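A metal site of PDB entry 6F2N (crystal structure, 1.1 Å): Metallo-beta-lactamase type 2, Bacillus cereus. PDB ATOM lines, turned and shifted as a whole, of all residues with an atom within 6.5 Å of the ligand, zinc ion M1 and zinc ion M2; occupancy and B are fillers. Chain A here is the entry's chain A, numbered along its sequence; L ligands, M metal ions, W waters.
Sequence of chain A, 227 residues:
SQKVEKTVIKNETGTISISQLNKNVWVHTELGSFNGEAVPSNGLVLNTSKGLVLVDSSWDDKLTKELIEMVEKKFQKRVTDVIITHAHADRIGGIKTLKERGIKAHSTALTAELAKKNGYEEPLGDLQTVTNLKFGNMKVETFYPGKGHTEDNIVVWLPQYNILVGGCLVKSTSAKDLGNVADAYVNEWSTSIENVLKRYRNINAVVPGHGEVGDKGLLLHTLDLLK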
ATOM      1  N   VAL A  39      23.404 -17.318  14.165  1.00  0.00           N
ATOM      2  CA  VAL A  39      22.236 -16.803  14.874  1.00  0.00           C
ATOM      3  C   VAL A  39      22.349 -15.294  14.777  1.00  0.00           C
ATOM      4  O   VAL A  39      23.258 -14.713  15.405  1.00  0.00           O
ATOM      5  CB  VAL A  39      22.198 -17.262  16.349  1.00  0.00           C
ATOM      6  CG1 VAL A  39      20.952 -16.643  17.078  1.00  0.00           C
ATOM      7  CG2 VAL A  39      22.200 -18.778  16.476  1.00  0.00           C
ATOM      8  N   PRO A  40      21.449 -14.619  14.061  1.00  0.00           N
ATOM      9  CA  PRO A  40      21.478 -13.150  14.038  1.00  0.00           C
ATOM     10  C   PRO A  40      20.892 -12.546  15.275  1.00  0.00           C
ATOM     11  O   PRO A  40      20.051 -13.139  15.939  1.00  0.00           O
ATOM     12  CB  PRO A  40      20.596 -12.810  12.839  1.00  0.00           C
ATOM     13  CG  PRO A  40      19.583 -13.807  12.913  1.00  0.00           C
ATOM     14  CD  PRO A  40      20.337 -15.107  13.260  1.00  0.00           C
ATOM     15  N   SER A  41      21.349 -11.332  15.576  1.00  0.00           N
ATOM     16  CA  SER A  41      20.780 -10.587  16.668  1.00  0.00           C
ATOM     17  C   SER A  41      20.781  -9.114  16.336  1.00  0.00           C
ATOM     18  O   SER A  41      21.598  -8.649  15.529  1.00  0.00           O
ATOM     19  CB  SER A  41      21.565 -10.824  17.949  1.00  0.00           C
ATOM     20  OG  SER A  41      22.907 -10.416  17.760  1.00  0.00           O
ATOM     21  N   TRP A  59      27.663 -10.432  20.457  1.00  0.00           N
ATOM     22  CA  TRP A  59      27.939 -11.746  21.023  1.00  0.00           C
ATOM     23  C   TRP A  59      29.269 -11.852  21.712  1.00  0.00           C
ATOM     24  O   TRP A  59      29.406 -12.718  22.592  1.00  0.00           O
ATOM     25  CB  TRP A  59      27.871 -12.798  19.908  1.00  0.00           C
ATOM     26  CG  TRP A  59      26.569 -12.918  19.242  1.00  0.00           C
ATOM     27  CD1 TRP A  59      26.132 -12.234  18.110  1.00  0.00           C
ATOM     28  CD2 TRP A  59      25.484 -13.758  19.656  1.00  0.00           C
ATOM     29  NE1 TRP A  59      24.846 -12.683  17.778  1.00  0.00           N
ATOM     30  CE2 TRP A  59      24.437 -13.608  18.709  1.00  0.00           C
ATOM     31  CE3 TRP A  59      25.321 -14.712  20.712  1.00  0.00           C
ATOM     32  CZ2 TRP A  59      23.245 -14.338  18.773  1.00  0.00           C
ATOM     33  CZ3 TRP A  59      24.131 -15.400  20.773  1.00  0.00           C
ATOM     34  CH2 TRP A  59      23.124 -15.255  19.785  1.00  0.00           C
ATOM     35  N   HIS A  86      19.795  -7.147  28.805  1.00  0.00           N
ATOM     36  CA  HIS A  86      19.797  -8.265  29.762  1.00  0.00           C
ATOM     37  C   HIS A  86      21.198  -8.875  29.715  1.00  0.00           C
ATOM     38  O   HIS A  86      22.054  -8.469  28.961  1.00  0.00           O
ATOM     39  CB  HIS A  86      18.678  -9.292  29.595  1.00  0.00           C
ATOM     40  CG  HIS A  86      18.727 -10.130  28.369  1.00  0.00           C
ATOM     41  ND1 HIS A  86      18.222  -9.715  27.160  1.00  0.00           N
ATOM     42  CD2 HIS A  86      19.051 -11.444  28.185  1.00  0.00           C
ATOM     43  CE1 HIS A  86      18.370 -10.702  26.304  1.00  0.00           C
ATOM     44  NE2 HIS A  86      18.825 -11.771  26.885  1.00  0.00           N
ATOM     45  N   ALA A  87      21.436  -9.836  30.594  1.00  0.00           N
ATOM     46  CA  ALA A  87      22.782 -10.384  30.861  1.00  0.00           C
ATOM     47  C   ALA A  87      23.153 -11.641  30.069  1.00  0.00           C
ATOM     48  O   ALA A  87      24.256 -12.160  30.341  1.00  0.00           O
ATOM     49  CB  ALA A  87      23.003 -10.592  32.355  1.00  0.00           C
ATOM     50  N   HIS A  88      22.543 -11.916  28.967  1.00  0.00           N
ATOM     51  CA  HIS A  88      22.979 -12.995  28.055  1.00  0.00           C
ATOM     52  C   HIS A  88      24.056 -12.458  27.040  1.00  0.00           C
ATOM     53  O   HIS A  88      24.147 -11.303  26.746  1.00  0.00           O
ATOM     54  CB  HIS A  88      21.790 -13.566  27.253  1.00  0.00           C
ATOM     55  CG  HIS A  88      20.870 -14.487  28.023  1.00  0.00           C
ATOM     56  ND1 HIS A  88      19.584 -14.745  27.614  1.00  0.00           N
ATOM     57  CD2 HIS A  88      21.086 -15.263  29.108  1.00  0.00           C
ATOM     58  CE1 HIS A  88      19.033 -15.635  28.432  1.00  0.00           C
ATOM     59  NE2 HIS A  88      19.938 -15.978  29.335  1.00  0.00           N
ATOM     60  N   ALA A  89      24.767 -13.407  26.426  1.00  0.00           N
ATOM     61  CA  ALA A  89      25.917 -13.083  25.574  1.00  0.00           C
ATOM     62  C   ALA A  89      25.573 -12.195  24.373  1.00  0.00           C
ATOM     63  O   ALA A  89      26.409 -11.370  23.961  1.00  0.00           O
ATOM     64  CB  ALA A  89      26.594 -14.346  25.083  1.00  0.00           C
ATOM     65  N   ASP A  90      24.448 -12.403  23.728  1.00  0.00           N
ATOM     66  CA  ASP A  90      24.061 -11.608  22.577  1.00  0.00           C
ATOM     67  C   ASP A  90      24.008 -10.157  22.915  1.00  0.00           C
ATOM     68  O   ASP A  90      24.223  -9.313  22.051  1.00  0.00           O
ATOM     69  CB  ASP A  90      22.786 -12.074  21.874  1.00  0.00           C
ATOM     70  CG  ASP A  90      21.539 -12.073  22.752  1.00  0.00           C
ATOM     71  OD1 ASP A  90      21.616 -12.262  23.980  1.00  0.00           O
ATOM     72  OD2 ASP A  90      20.432 -11.976  22.167  1.00  0.00           O
ATOM     73  N   ARG A  91      23.606  -9.841  24.160  1.00  0.00           N
ATOM     74  CA  ARG A  91      23.520  -8.463  24.612  1.00  0.00           C
ATOM     75  C   ARG A  91      24.776  -7.876  25.245  1.00  0.00           C
ATOM     76  O   ARG A  91      25.120  -6.720  25.021  1.00  0.00           O
ATOM     77  CB  ARG A  91      22.440  -8.345  25.695  1.00  0.00           C
ATOM     78  CG  ARG A  91      21.113  -9.024  25.399  1.00  0.00           C
ATOM     79  CD  ARG A  91      20.330  -8.304  24.319  1.00  0.00           C
ATOM     80  NE  ARG A  91      20.305  -9.071  23.076  1.00  0.00           N
ATOM     81  CZ  ARG A  91      19.946  -8.586  21.896  1.00  0.00           C
ATOM     82  NH1 ARG A  91      19.597  -7.308  21.783  1.00  0.00           N
ATOM     83  NH2 ARG A  91      19.953  -9.364  20.827  1.00  0.00           N
ATOM     84  N   HIS A 149      11.571 -13.202  29.063  1.00  0.00           N
ATOM     85  CA  HIS A 149      12.649 -13.966  28.474  1.00  0.00           C
ATOM     86  C   HIS A 149      13.732 -14.274  29.483  1.00  0.00           C
ATOM     87  O   HIS A 149      14.307 -15.354  29.497  1.00  0.00           O
ATOM     88  CB  HIS A 149      13.192 -13.207  27.271  1.00  0.00           C
ATOM     89  CG  HIS A 149      14.500 -13.703  26.793  1.00  0.00           C
ATOM     90  ND1 HIS A 149      14.663 -14.900  26.115  1.00  0.00           N
ATOM     91  CD2 HIS A 149      15.723 -13.185  26.944  1.00  0.00           C
ATOM     92  CE1 HIS A 149      15.953 -15.047  25.839  1.00  0.00           C
ATOM     93  NE2 HIS A 149      16.650 -14.003  26.342  1.00  0.00           N
ATOM     94  N   THR A 150      14.064 -13.287  30.315  1.00  0.00           N
ATOM     95  CA  THR A 150      14.894 -13.416  31.482  1.00  0.00           C
ATOM     96  C   THR A 150      14.244 -12.677  32.631  1.00  0.00           C
ATOM     97  O   THR A 150      13.312 -11.903  32.463  1.00  0.00           O
ATOM     98  CB  THR A 150      16.313 -12.927  31.270  1.00  0.00           C
ATOM     99  OG1 THR A 150      16.226 -11.547  30.909  1.00  0.00           O
ATOM    100  CG2 THR A 150      17.052 -13.756  30.238  1.00  0.00           C
ATOM    101  N   GLY A 167      13.904  -6.007  22.440  1.00  0.00           N
ATOM    102  CA  GLY A 167      14.879  -6.934  22.859  1.00  0.00           C
ATOM    103  C   GLY A 167      14.331  -8.351  22.845  1.00  0.00           C
ATOM    104  O   GLY A 167      13.372  -8.667  22.156  1.00  0.00           O
ATOM    105  N   CYS A 168      14.937  -9.216  23.645  1.00  0.00           N
ATOM    106  CA  CYS A 168      14.623 -10.597  23.553  1.00  0.00           C
ATOM    107  C   CYS A 168      13.330 -10.981  24.265  1.00  0.00           C
ATOM    108  O   CYS A 168      12.845 -12.090  24.072  1.00  0.00           O
ATOM    109  CB  CYS A 168      15.809 -11.411  23.951  1.00  0.00           C
ATOM    110  SG  CYS A 168      17.341 -10.880  23.002  1.00  0.00           S
ATOM    111  N   LEU A 169      12.733 -10.034  24.959  1.00  0.00           N
ATOM    112  CA  LEU A 169      11.341 -10.155  25.437  1.00  0.00           C
ATOM    113  C   LEU A 169      10.359 -10.305  24.288  1.00  0.00           C
ATOM    114  O   LEU A 169       9.245 -10.861  24.479  1.00  0.00           O
ATOM    115  CB  LEU A 169      11.010  -8.865  26.223  1.00  0.00           C
ATOM    116  CG  LEU A 169       9.677  -8.812  26.889  1.00  0.00           C
ATOM    117  CD1 LEU A 169       9.580  -9.711  28.150  1.00  0.00           C
ATOM    118  CD2 LEU A 169       9.351  -7.360  27.305  1.00  0.00           C
ATOM    119  N   LYS A 171       9.436 -11.566  20.434  1.00  0.00           N
ATOM    120  CA  LYS A 171       9.781 -12.468  19.350  1.00  0.00           C
ATOM    121  C   LYS A 171       9.368 -11.921  17.994  1.00  0.00           C
ATOM    122  O   LYS A 171       8.323 -11.274  17.866  1.00  0.00           O
ATOM    123  CB  LYS A 171       9.062 -13.802  19.616  1.00  0.00           C
ATOM    124  CG  LYS A 171       9.502 -14.468  20.927  1.00  0.00           C
ATOM    125  CD  LYS A 171      10.995 -14.882  20.862  1.00  0.00           C
ATOM    126  CE  LYS A 171      11.534 -15.642  21.979  1.00  0.00           C
ATOM    127  NZ  LYS A 171      12.930 -16.130  21.732  1.00  0.00           N
ATOM    128  N   LEU A 178       9.284 -20.110  21.665  1.00  0.00           N
ATOM    129  CA  LEU A 178       9.915 -19.147  22.548  1.00  0.00           C
ATOM    130  C   LEU A 178      11.425 -19.252  22.592  1.00  0.00           C
ATOM    131  O   LEU A 178      12.050 -18.442  23.236  1.00  0.00           O
ATOM    132  CB  LEU A 178       9.359 -19.338  23.942  1.00  0.00           C
ATOM    133  CG  LEU A 178       7.838 -19.071  24.088  1.00  0.00           C
ATOM    134  CD1 LEU A 178       7.344 -19.583  25.417  1.00  0.00           C
ATOM    135  CD2 LEU A 178       7.571 -17.554  23.898  1.00  0.00           C
ATOM    136  N   GLY A 179      12.002 -20.242  21.964  1.00  0.00           N
ATOM    137  CA  GLY A 179      13.426 -20.356  21.970  1.00  0.00           C
ATOM    138  C   GLY A 179      13.972 -20.881  23.293  1.00  0.00           C
ATOM    139  O   GLY A 179      13.357 -21.690  23.990  1.00  0.00           O
ATOM    140  N   ASN A 180      15.132 -20.395  23.684  1.00  0.00           N
ATOM    141  CA  ASN A 180      15.786 -20.871  24.893  1.00  0.00           C
ATOM    142  C   ASN A 180      15.085 -20.245  26.098  1.00  0.00           C
ATOM    143  O   ASN A 180      15.151 -19.023  26.314  1.00  0.00           O
ATOM    144  CB  ASN A 180      17.283 -20.574  24.898  1.00  0.00           C
ATOM    145  CG  ASN A 180      18.019 -21.287  26.035  1.00  0.00           C
ATOM    146  OD1 ASN A 180      17.565 -21.296  27.149  1.00  0.00           O
ATOM    147  ND2 ASN A 180      19.207 -21.854  25.730  1.00  0.00           N
ATOM    148  N   VAL A 181      14.455 -21.093  26.893  1.00  0.00           N
ATOM    149  CA  VAL A 181      13.646 -20.706  28.035  1.00  0.00           C
ATOM    150  C   VAL A 181      14.293 -21.150  29.343  1.00  0.00           C
ATOM    151  O   VAL A 181      13.670 -21.026  30.404  1.00  0.00           O
ATOM    152  CB  VAL A 181      12.182 -21.157  27.922  1.00  0.00           C
ATOM    153  CG1 VAL A 181      11.445 -20.486  26.791  1.00  0.00           C
ATOM    154  CG2 VAL A 181      12.111 -22.744  27.814  1.00  0.00           C
ATOM    155  N   ALA A 182      15.579 -21.493  29.305  1.00  0.00           N
ATOM    156  CA  ALA A 182      16.252 -21.919  30.521  1.00  0.00           C
ATOM    157  C   ALA A 182      16.177 -20.831  31.610  1.00  0.00           C
ATOM    158  O   ALA A 182      16.083 -21.138  32.818  1.00  0.00           O
ATOM    159  CB  ALA A 182      17.734 -22.207  30.233  1.00  0.00           C
ATOM    160  N   ASP A 183      16.283 -19.581  31.212  1.00  0.00           N
ATOM    161  CA  ASP A 183      16.333 -18.471  32.129  1.00  0.00           C
ATOM    162  C   ASP A 183      15.040 -17.681  32.158  1.00  0.00           C
ATOM    163  O   ASP A 183      15.004 -16.583  32.734  1.00  0.00           O
ATOM    164  CB  ASP A 183      17.544 -17.584  31.794  1.00  0.00           C
ATOM    165  CG  ASP A 183      18.858 -18.311  31.964  1.00  0.00           C
ATOM    166  OD1 ASP A 183      19.001 -19.093  32.905  1.00  0.00           O
ATOM    167  OD2 ASP A 183      19.746 -18.038  31.174  1.00  0.00           O
ATOM    168  N   GLY A 209      14.688  -8.760  19.572  1.00  0.00           N
ATOM    169  CA  GLY A 209      16.085  -9.085  19.808  1.00  0.00           C
ATOM    170  C   GLY A 209      16.723  -9.856  18.683  1.00  0.00           C
ATOM    171  O   GLY A 209      17.942  -9.776  18.460  1.00  0.00           O
ATOM    172  N   HIS A 210      15.909 -10.628  17.957  1.00  0.00           N
ATOM    173  CA  HIS A 210      16.327 -11.430  16.828  1.00  0.00           C
ATOM    174  C   HIS A 210      15.228 -11.348  15.763  1.00  0.00           C
ATOM    175  O   HIS A 210      14.042 -11.411  16.095  1.00  0.00           O
ATOM    176  CB  HIS A 210      16.589 -12.927  17.273  1.00  0.00           C
ATOM    177  CG  HIS A 210      17.516 -13.083  18.486  1.00  0.00           C
ATOM    178  ND1 HIS A 210      18.884 -13.196  18.421  1.00  0.00           N
ATOM    179  CD2 HIS A 210      17.231 -13.079  19.836  1.00  0.00           C
ATOM    180  CE1 HIS A 210      19.398 -13.212  19.638  1.00  0.00           C
ATOM    181  NE2 HIS A 210      18.412 -13.166  20.529  1.00  0.00           N
HETATM  182  C1  LIG L   1      19.420 -17.994  26.046  1.00  0.00           C
HETATM  183  C2  LIG L   1      20.482 -18.398  26.811  1.00  0.00           C
HETATM  184  C3  LIG L   1      21.747 -18.303  26.324  1.00  0.00           C
HETATM  185  C4  LIG L   1      21.972 -17.814  25.046  1.00  0.00           C
HETATM  186  C5  LIG L   1      20.923 -17.380  24.234  1.00  0.00           C
HETATM  187  C6  LIG L   1      21.204 -16.885  22.820  1.00  0.00           C
HETATM  188  C7  LIG L   1      20.439 -17.599  21.703  1.00  0.00           C
HETATM  189  C8  LIG L   1      19.599 -16.901  20.883  1.00  0.00           C
HETATM  190  C9  LIG L   1      18.876 -17.522  19.840  1.00  0.00           C
HETATM  191  C10 LIG L   1      18.019 -16.809  18.956  1.00  0.00           C
HETATM  192  C11 LIG L   1      17.329 -17.454  17.965  1.00  0.00           C
HETATM  193  C12 LIG L   1      17.485 -18.828  17.781  1.00  0.00           C
HETATM  194  C13 LIG L   1      18.250 -15.585  23.665  1.00  0.00           C
HETATM  195  O1  LIG L   1      16.743 -14.132  22.691  1.00  0.00           O
HETATM  196  C14 LIG L   1      17.005 -15.332  22.905  1.00  0.00           C
HETATM  197  C15 LIG L   1      18.319 -19.555  18.596  1.00  0.00           C
HETATM  198  C16 LIG L   1      19.031 -18.919  19.646  1.00  0.00           C
HETATM  199  C17 LIG L   1      19.899 -19.627  20.508  1.00  0.00           C
HETATM  200  C18 LIG L   1      20.578 -18.967  21.506  1.00  0.00           C
HETATM  201  C19 LIG L   1      18.484 -16.883  24.028  1.00  0.00           C
HETATM  202  C20 LIG L   1      19.618 -17.448  24.770  1.00  0.00           C
HETATM  203  O2  LIG L   1      16.128 -16.218  22.646  1.00  0.00           O
HETATM  204  S1  LIG L   1      19.371 -14.286  24.062  1.00  0.00           S
HETATM  205 ZN    ZN M   1      18.636 -13.700  26.194  1.00  0.00          ZN
HETATM  206 ZN    ZN M   2      18.483 -12.770  22.537  1.00  0.00          ZN
HETATM  207  O   HOH W   1      16.191 -18.540  21.585  1.00  0.00           O
HETATM  208  O   HOH W   2      18.286 -15.573  15.472  1.00  0.00           O
HETATM  209  O   HOH W   3      14.106 -13.582  22.046  1.00  0.00           O
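An oxygen (O2) of the ligand is in salt-bridge range of the side-chain amino group (NZ) of Lys 171 (3.3 Å).
N of Ala 182 is in hydrogen-bond range of OD1 of Asn 180, 2.9 Å away.
The side-chain sulfur (SG) of Cys 168 lies close to the guanidinium group (NE) of Arg 91, at 3.5 Å.
The backbone carbonyl oxygen (O) of Pro 40 lies within hydrogen-bond range of a ring nitrogen (ND1) of His 210, 2.7 Å away.
The backbone carbonyl oxygen of Leu 178 is in hydrogen-bond range of the side-chain amino group of Lys 171 (2.9 Å).
NE of Arg 91 is in salt-bridge range of OD1 of Asp 90 (3.6 Å).
The indole nitrogen of Trp 59 sits at hydrogen-bond distance from the side-chain hydroxyl of Ser 41 (3.0 Å).
A ring nitrogen (NE2) of His 88 lies within hydrogen-bond range of the side-chain carboxylate (OD2) of Asp 183 (2.8 Å).
Residues that only touch the ligand: Val 39 (3.5 Å), Trp 59 (3.9 Å) and Asn 180 (3.5 Å).
Hydrophobic or aromatic side chains that line the ligand: Val 39, Trp 59, His 88, His 149 and His 210.
Of the 24 residues printed, 10 come within 4 Å of the ligand.
Along chain A the residues within 4 Å of the ligand span positions 39 to 210.
The nearest printed residue that does not touch the ligand is Asp 183 (4.4 Å).
Four residues have an atom within 4 Å of zinc ion M1: His 86, His 88, Asp 90 and His 149.
Along chain A the residues within 4 Å of zinc ion M1 span positions 86 to 149.
The nearest printed residue that does not touch zinc ion M1 is Cys 168 (4.3 Å).
Three residues have an atom within 4 Å of zinc ion M2: Asp 90, Cys 168 and His 210.
Along chain A the residues within 4 Å of zinc ion M2 span positions 90 to 210.
The nearest printed residue that does not touch zinc ion M2 is Arg 91 (4.1 Å).
Zinc ion M1 is bound by a ring nitrogen (ND1) of His 88 (2.0 Å), a ring nitrogen (NE2) of His 149 (2.0 Å), a ring nitrogen (NE2) of His 86 (2.1 Å) and a sulfur (S1) of the ligand (2.3 Å).
Zinc ion M2 is bound by NE2 of His 210, OD2 of Asp 90, O1 of the ligand, SG of Cys 168 and S1 of the ligand.
Water W1 lies within hydrogen-bond range of O2 of the ligand (2.6 Å) and N of Asn 180 (3.0 Å).
Water W3 lies within hydrogen-bond range of O of Cys 168 (2.8 Å), NZ of Lys 171 (2.8 Å) and O2 of the ligand (3.4 Å).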
